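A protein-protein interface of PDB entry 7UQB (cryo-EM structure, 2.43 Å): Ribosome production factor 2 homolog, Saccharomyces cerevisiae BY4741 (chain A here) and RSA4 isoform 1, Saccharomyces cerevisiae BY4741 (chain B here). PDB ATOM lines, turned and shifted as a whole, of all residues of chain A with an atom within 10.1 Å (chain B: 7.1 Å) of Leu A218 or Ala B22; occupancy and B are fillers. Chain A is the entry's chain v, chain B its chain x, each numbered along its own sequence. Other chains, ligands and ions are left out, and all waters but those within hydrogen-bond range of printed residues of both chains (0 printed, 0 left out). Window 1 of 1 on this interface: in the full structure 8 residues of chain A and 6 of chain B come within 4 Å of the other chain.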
ATOM      1  N   SER A 208     -25.555   1.286  22.545  1.00  0.00           N
ATOM      2  CA  SER A 208     -25.963   0.281  21.576  1.00  0.00           C
ATOM      3  C   SER A 208     -26.079   0.920  20.200  1.00  0.00           C
ATOM      4  O   SER A 208     -26.705   1.973  20.050  1.00  0.00           O
ATOM      5  CB  SER A 208     -27.288  -0.366  21.981  1.00  0.00           C
ATOM      6  OG  SER A 208     -28.295   0.608  22.183  1.00  0.00           O
ATOM      7  N   TYR A 209     -25.465   0.285  19.205  1.00  0.00           N
ATOM      8  CA  TYR A 209     -25.526   0.738  17.825  1.00  0.00           C
ATOM      9  C   TYR A 209     -26.044  -0.393  16.950  1.00  0.00           C
ATOM     10  O   TYR A 209     -25.865  -1.572  17.266  1.00  0.00           O
ATOM     11  CB  TYR A 209     -24.156   1.195  17.303  1.00  0.00           C
ATOM     12  CG  TYR A 209     -23.476   2.252  18.141  1.00  0.00           C
ATOM     13  CD1 TYR A 209     -23.775   3.598  17.977  1.00  0.00           C
ATOM     14  CD2 TYR A 209     -22.521   1.904  19.089  1.00  0.00           C
ATOM     15  CE1 TYR A 209     -23.148   4.568  18.740  1.00  0.00           C
ATOM     16  CE2 TYR A 209     -21.892   2.864  19.853  1.00  0.00           C
ATOM     17  CZ  TYR A 209     -22.208   4.194  19.676  1.00  0.00           C
ATOM     18  OH  TYR A 209     -21.577   5.150  20.437  1.00  0.00           O
ATOM     19  N   LYS A 210     -26.693  -0.016  15.850  1.00  0.00           N
ATOM     20  CA  LYS A 210     -27.194  -0.996  14.894  1.00  0.00           C
ATOM     21  C   LYS A 210     -26.037  -1.783  14.291  1.00  0.00           C
ATOM     22  O   LYS A 210     -25.045  -1.204  13.839  1.00  0.00           O
ATOM     23  CB  LYS A 210     -27.991  -0.291  13.798  1.00  0.00           C
ATOM     24  CG  LYS A 210     -28.617  -1.221  12.781  1.00  0.00           C
ATOM     25  CD  LYS A 210     -29.807  -1.957  13.365  1.00  0.00           C
ATOM     26  CE  LYS A 210     -30.423  -2.887  12.334  1.00  0.00           C
ATOM     27  NZ  LYS A 210     -30.786  -2.163  11.085  1.00  0.00           N
ATOM     28  N   SER A 211     -26.169  -3.110  14.282  1.00  0.00           N
ATOM     29  CA  SER A 211     -25.051  -3.964  13.895  1.00  0.00           C
ATOM     30  C   SER A 211     -24.971  -4.180  12.390  1.00  0.00           C
ATOM     31  O   SER A 211     -23.870  -4.354  11.860  1.00  0.00           O
ATOM     32  CB  SER A 211     -25.152  -5.316  14.602  1.00  0.00           C
ATOM     33  OG  SER A 211     -26.183  -6.106  14.041  1.00  0.00           O
ATOM     34  N   ASP A 212     -26.120  -4.222  11.708  1.00  0.00           N
ATOM     35  CA  ASP A 212     -26.239  -4.423  10.263  1.00  0.00           C
ATOM     36  C   ASP A 212     -25.734  -5.795   9.818  1.00  0.00           C
ATOM     37  O   ASP A 212     -25.664  -6.077   8.617  1.00  0.00           O
ATOM     38  CB  ASP A 212     -25.510  -3.312   9.496  1.00  0.00           C
ATOM     39  CG  ASP A 212     -26.072  -3.098   8.105  1.00  0.00           C
ATOM     40  OD1 ASP A 212     -27.202  -3.565   7.845  1.00  0.00           O
ATOM     41  OD2 ASP A 212     -25.383  -2.474   7.273  1.00  0.00           O
ATOM     42  N   GLN A 213     -25.392  -6.658  10.770  1.00  0.00           N
ATOM     43  CA  GLN A 213     -25.019  -8.038  10.490  1.00  0.00           C
ATOM     44  C   GLN A 213     -25.834  -9.050  11.274  1.00  0.00           C
ATOM     45  O   GLN A 213     -26.105 -10.136  10.756  1.00  0.00           O
ATOM     46  CB  GLN A 213     -23.529  -8.267  10.785  1.00  0.00           C
ATOM     47  CG  GLN A 213     -22.590  -7.647   9.760  1.00  0.00           C
ATOM     48  CD  GLN A 213     -21.130  -7.921  10.062  1.00  0.00           C
ATOM     49  OE1 GLN A 213     -20.794  -8.478  11.107  1.00  0.00           O
ATOM     50  NE2 GLN A 213     -20.253  -7.528   9.146  1.00  0.00           N
ATOM     51  N   GLY A 214     -26.229  -8.727  12.501  1.00  0.00           N
ATOM     52  CA  GLY A 214     -27.117  -9.548  13.292  1.00  0.00           C
ATOM     53  C   GLY A 214     -28.570  -9.129  13.256  1.00  0.00           C
ATOM     54  O   GLY A 214     -29.358  -9.618  14.075  1.00  0.00           O
ATOM     55  N   GLY A 215     -28.952  -8.244  12.341  1.00  0.00           N
ATOM     56  CA  GLY A 215     -30.326  -7.814  12.231  1.00  0.00           C
ATOM     57  C   GLY A 215     -30.681  -6.711  13.211  1.00  0.00           C
ATOM     58  O   GLY A 215     -29.841  -6.161  13.927  1.00  0.00           O
ATOM     59  N   LYS A 216     -31.972  -6.389  13.230  1.00  0.00           N
ATOM     60  CA  LYS A 216     -32.497  -5.369  14.126  1.00  0.00           C
ATOM     61  C   LYS A 216     -32.774  -5.900  15.525  1.00  0.00           C
ATOM     62  O   LYS A 216     -33.165  -5.118  16.399  1.00  0.00           O
ATOM     63  CB  LYS A 216     -33.770  -4.760  13.533  1.00  0.00           C
ATOM     64  CG  LYS A 216     -34.761  -5.782  13.004  1.00  0.00           C
ATOM     65  CD  LYS A 216     -35.805  -5.127  12.114  1.00  0.00           C
ATOM     66  CE  LYS A 216     -36.669  -4.149  12.894  1.00  0.00           C
ATOM     67  NZ  LYS A 216     -37.479  -4.840  13.933  1.00  0.00           N
ATOM     68  N   ARG A 217     -32.584  -7.198  15.760  1.00  0.00           N
ATOM     69  CA  ARG A 217     -32.777  -7.779  17.080  1.00  0.00           C
ATOM     70  C   ARG A 217     -31.490  -7.875  17.890  1.00  0.00           C
ATOM     71  O   ARG A 217     -31.560  -7.964  19.120  1.00  0.00           O
ATOM     72  CB  ARG A 217     -33.397  -9.177  16.958  1.00  0.00           C
ATOM     73  CG  ARG A 217     -34.544  -9.265  15.958  1.00  0.00           C
ATOM     74  CD  ARG A 217     -35.719  -8.393  16.365  1.00  0.00           C
ATOM     75  NE  ARG A 217     -36.398  -8.907  17.547  1.00  0.00           N
ATOM     76  CZ  ARG A 217     -37.437  -9.730  17.514  1.00  0.00           C
ATOM     77  NH1 ARG A 217     -37.950 -10.152  16.369  1.00  0.00           N
ATOM     78  NH2 ARG A 217     -37.975 -10.142  18.659  1.00  0.00           N
ATOM     79  N   LEU A 218     -30.329  -7.861  17.240  1.00  0.00           N
ATOM     80  CA  LEU A 218     -29.040  -7.983  17.923  1.00  0.00           C
ATOM     81  C   LEU A 218     -28.170  -6.769  17.626  1.00  0.00           C
ATOM     82  O   LEU A 218     -27.536  -6.702  16.558  1.00  0.00           O
ATOM     83  CB  LEU A 218     -28.326  -9.264  17.500  1.00  0.00           C
ATOM     84  CG  LEU A 218     -29.121 -10.556  17.684  1.00  0.00           C
ATOM     85  CD1 LEU A 218     -28.291 -11.753  17.259  1.00  0.00           C
ATOM     86  CD2 LEU A 218     -29.586 -10.702  19.122  1.00  0.00           C
ATOM     87  N   PRO A 219     -28.102  -5.794  18.526  1.00  0.00           N
ATOM     88  CA  PRO A 219     -27.262  -4.617  18.292  1.00  0.00           C
ATOM     89  C   PRO A 219     -25.808  -4.869  18.671  1.00  0.00           C
ATOM     90  O   PRO A 219     -25.443  -5.902  19.232  1.00  0.00           O
ATOM     91  CB  PRO A 219     -27.891  -3.564  19.206  1.00  0.00           C
ATOM     92  CG  PRO A 219     -28.411  -4.362  20.351  1.00  0.00           C
ATOM     93  CD  PRO A 219     -28.891  -5.668  19.762  1.00  0.00           C
ATOM     94  N   ARG A 220     -24.976  -3.882  18.350  1.00  0.00           N
ATOM     95  CA  ARG A 220     -23.570  -3.862  18.722  1.00  0.00           C
ATOM     96  C   ARG A 220     -23.393  -3.008  19.972  1.00  0.00           C
ATOM     97  O   ARG A 220     -24.019  -1.954  20.108  1.00  0.00           O
ATOM     98  CB  ARG A 220     -22.716  -3.315  17.575  1.00  0.00           C
ATOM     99  CG  ARG A 220     -21.249  -3.074  17.903  1.00  0.00           C
ATOM    100  CD  ARG A 220     -20.457  -4.368  18.011  1.00  0.00           C
ATOM    101  NE  ARG A 220     -19.024  -4.102  18.084  1.00  0.00           N
ATOM    102  CZ  ARG A 220     -18.082  -5.036  18.096  1.00  0.00           C
ATOM    103  NH1 ARG A 220     -18.384  -6.322  18.060  1.00  0.00           N
ATOM    104  NH2 ARG A 220     -16.805  -4.669  18.148  1.00  0.00           N
ATOM    105  N   ILE A 221     -22.543  -3.469  20.883  1.00  0.00           N
ATOM    106  CA  ILE A 221     -22.334  -2.820  22.174  1.00  0.00           C
ATOM    107  C   ILE A 221     -21.006  -2.078  22.151  1.00  0.00           C
ATOM    108  O   ILE A 221     -20.031  -2.547  21.553  1.00  0.00           O
ATOM    109  CB  ILE A 221     -22.379  -3.858  23.313  1.00  0.00           C
ATOM    110  CG1 ILE A 221     -23.725  -4.587  23.314  1.00  0.00           C
ATOM    111  CG2 ILE A 221     -22.142  -3.206  24.663  1.00  0.00           C
ATOM    112  CD1 ILE A 221     -24.917  -3.670  23.512  1.00  0.00           C
ATOM    113  N   GLU B  20     -29.690 -20.046  23.527  1.00  0.00           N
ATOM    114  CA  GLU B  20     -29.075 -20.005  22.210  1.00  0.00           C
ATOM    115  C   GLU B  20     -29.472 -18.715  21.503  1.00  0.00           C
ATOM    116  O   GLU B  20     -30.629 -18.291  21.562  1.00  0.00           O
ATOM    117  CB  GLU B  20     -29.473 -21.226  21.375  1.00  0.00           C
ATOM    118  CG  GLU B  20     -30.969 -21.458  21.227  1.00  0.00           C
ATOM    119  CD  GLU B  20     -31.534 -20.852  19.958  1.00  0.00           C
ATOM    120  OE1 GLU B  20     -30.760 -20.244  19.190  1.00  0.00           O
ATOM    121  OE2 GLU B  20     -32.754 -20.988  19.722  1.00  0.00           O
ATOM    122  N   VAL B  21     -28.500 -18.089  20.847  1.00  0.00           N
ATOM    123  CA  VAL B  21     -28.693 -16.805  20.182  1.00  0.00           C
ATOM    124  C   VAL B  21     -28.937 -17.058  18.702  1.00  0.00           C
ATOM    125  O   VAL B  21     -28.188 -17.805  18.059  1.00  0.00           O
ATOM    126  CB  VAL B  21     -27.480 -15.883  20.392  1.00  0.00           C
ATOM    127  CG1 VAL B  21     -27.745 -14.510  19.799  1.00  0.00           C
ATOM    128  CG2 VAL B  21     -27.147 -15.775  21.870  1.00  0.00           C
ATOM    129  N   ALA B  22     -29.986 -16.443  18.162  1.00  0.00           N
ATOM    130  CA  ALA B  22     -30.330 -16.590  16.750  1.00  0.00           C
ATOM    131  C   ALA B  22     -29.523 -15.579  15.945  1.00  0.00           C
ATOM    132  O   ALA B  22     -29.830 -14.385  15.934  1.00  0.00           O
ATOM    133  CB  ALA B  22     -31.826 -16.398  16.539  1.00  0.00           C
ATOM    134  N   ILE B  23     -28.490 -16.059  15.260  1.00  0.00           N
ATOM    135  CA  ILE B  23     -27.589 -15.217  14.485  1.00  0.00           C
ATOM    136  C   ILE B  23     -27.536 -15.751  13.059  1.00  0.00           C
ATOM    137  O   ILE B  23     -27.622 -16.963  12.835  1.00  0.00           O
ATOM    138  CB  ILE B  23     -26.183 -15.158  15.123  1.00  0.00           C
ATOM    139  CG1 ILE B  23     -25.306 -14.122  14.417  1.00  0.00           C
ATOM    140  CG2 ILE B  23     -25.514 -16.529  15.136  1.00  0.00           C
ATOM    141  CD1 ILE B  23     -25.835 -12.717  14.525  1.00  0.00           C
ATOM    142  N   ILE B  24     -27.444 -14.838  12.095  1.00  0.00           N
ATOM    143  CA  ILE B  24     -27.314 -15.209  10.689  1.00  0.00           C
ATOM    144  C   ILE B  24     -25.957 -15.869  10.483  1.00  0.00           C
ATOM    145  O   ILE B  24     -24.925 -15.281  10.839  1.00  0.00           O
ATOM    146  CB  ILE B  24     -27.473 -13.989   9.770  1.00  0.00           C
ATOM    147  CG1 ILE B  24     -28.871 -13.387   9.907  1.00  0.00           C
ATOM    148  CG2 ILE B  24     -27.182 -14.371   8.325  1.00  0.00           C
ATOM    149  CD1 ILE B  24     -29.052 -12.094   9.145  1.00  0.00           C
ATOM    150  N   TYR B 101     -34.018 -15.576   5.890  1.00  0.00           N
ATOM    151  CA  TYR B 101     -33.527 -16.741   6.619  1.00  0.00           C
ATOM    152  C   TYR B 101     -34.325 -16.970   7.897  1.00  0.00           C
ATOM    153  O   TYR B 101     -34.814 -18.077   8.148  1.00  0.00           O
ATOM    154  CB  TYR B 101     -32.042 -16.577   6.940  1.00  0.00           C
ATOM    155  CG  TYR B 101     -31.508 -17.632   7.884  1.00  0.00           C
ATOM    156  CD1 TYR B 101     -31.213 -18.909   7.430  1.00  0.00           C
ATOM    157  CD2 TYR B 101     -31.298 -17.351   9.229  1.00  0.00           C
ATOM    158  CE1 TYR B 101     -30.731 -19.878   8.285  1.00  0.00           C
ATOM    159  CE2 TYR B 101     -30.816 -18.316  10.093  1.00  0.00           C
ATOM    160  CZ  TYR B 101     -30.533 -19.578   9.613  1.00  0.00           C
ATOM    161  OH  TYR B 101     -30.050 -20.545  10.465  1.00  0.00           O
ATOM    162  N   SER B 102     -34.473 -15.926   8.716  1.00  0.00           N
ATOM    163  CA  SER B 102     -35.171 -16.069   9.986  1.00  0.00           C
ATOM    164  C   SER B 102     -36.680 -16.169   9.813  1.00  0.00           C
ATOM    165  O   SER B 102     -37.368 -16.594  10.746  1.00  0.00           O
ATOM    166  CB  SER B 102     -34.831 -14.899  10.909  1.00  0.00           C
ATOM    167  OG  SER B 102     -35.284 -13.674  10.363  1.00  0.00           O
ATOM    168  N   LYS B 106     -35.222 -20.484   8.614  1.00  0.00           N
ATOM    169  CA  LYS B 106     -35.058 -20.927   9.999  1.00  0.00           C
ATOM    170  C   LYS B 106     -36.089 -21.973  10.418  1.00  0.00           C
ATOM    171  O   LYS B 106     -35.690 -22.979  11.030  1.00  0.00           O
ATOM    172  CB  LYS B 106     -35.053 -19.712  10.936  1.00  0.00           C
ATOM    173  CG  LYS B 106     -34.931 -20.057  12.411  1.00  0.00           C
ATOM    174  CD  LYS B 106     -34.932 -18.802  13.268  1.00  0.00           C
ATOM    175  CE  LYS B 106     -34.685 -19.129  14.730  1.00  0.00           C
ATOM    176  NZ  LYS B 106     -34.725 -17.910  15.582  1.00  0.00           N
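CD1 of Ile B24 touches O of Gln A213, at 3.9 Å.
CA of Gly A214 touches CD1 of Ile B23, at 3.6 Å.
CD1 of Leu A218 touches CG1 of Val B21, 3.8 Å away.
Ala B22 touches Leu A218.
CD1 of Leu A218 touches CD1 of Ile B23 (3.8 Å).
Of the printed residues of chain B, Gln A213 touches Ile B24 (3.9 Å).
Printed residues of chain B within 4 Å of Gly A214: Ile B23.
Of chain B, only Val B21 (3.8 Å), Ala B22 (3.3 Å) and Ile B23 (3.8 Å) come within 4 Å of Leu A218.
Arg A220 touches none of the printed residues of chain B.
Glu B20 touches none of the printed residues of chain A.
Ala B22 touches just one residue of chain A: Leu A218 (3.3 Å).
Ile B23 touches just these residues of chain A: Gly A214 (3.6 Å) and Leu A218 (3.8 Å).
Of the printed residues of chain A, Ile B24 touches Gln A213.
The nearest residue of chain A that does not touch Ala B22 is Gly A214 (5.1 Å).
The nearest printed residue of chain B that does not touch Gly A214 is Ile B24 (5.1 Å).
OG of Ser A211 sits close to N of Gln A213, 3.4 Å away.
The side-chain hydroxyl (OG) of Ser A211 is in hydrogen-bond range of the backbone NH (N) of Gly A214 (3.0 Å).
The side-chain hydroxyl (OG) of Ser A211 sits at hydrogen-bond distance from the backbone carbonyl oxygen (O) of Leu A218, 2.9 Å away.
Of the 8 printed residues of chain B, 4 touch a printed residue of chain A.
Hydrophobic or aromatic side chains of chain B within 4 Å of the printed part of chain A: Val B21, Ile B23 and Ile B24.
Of the 14 printed residues of chain A, 3 touch a printed residue of chain B.
Among the printed residues, 5 pairs touch across the chains.
Among the printed residues, no Asp or Glu carboxylate lies within 4 Å of a Lys or Arg side-chain nitrogen of the other chain.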
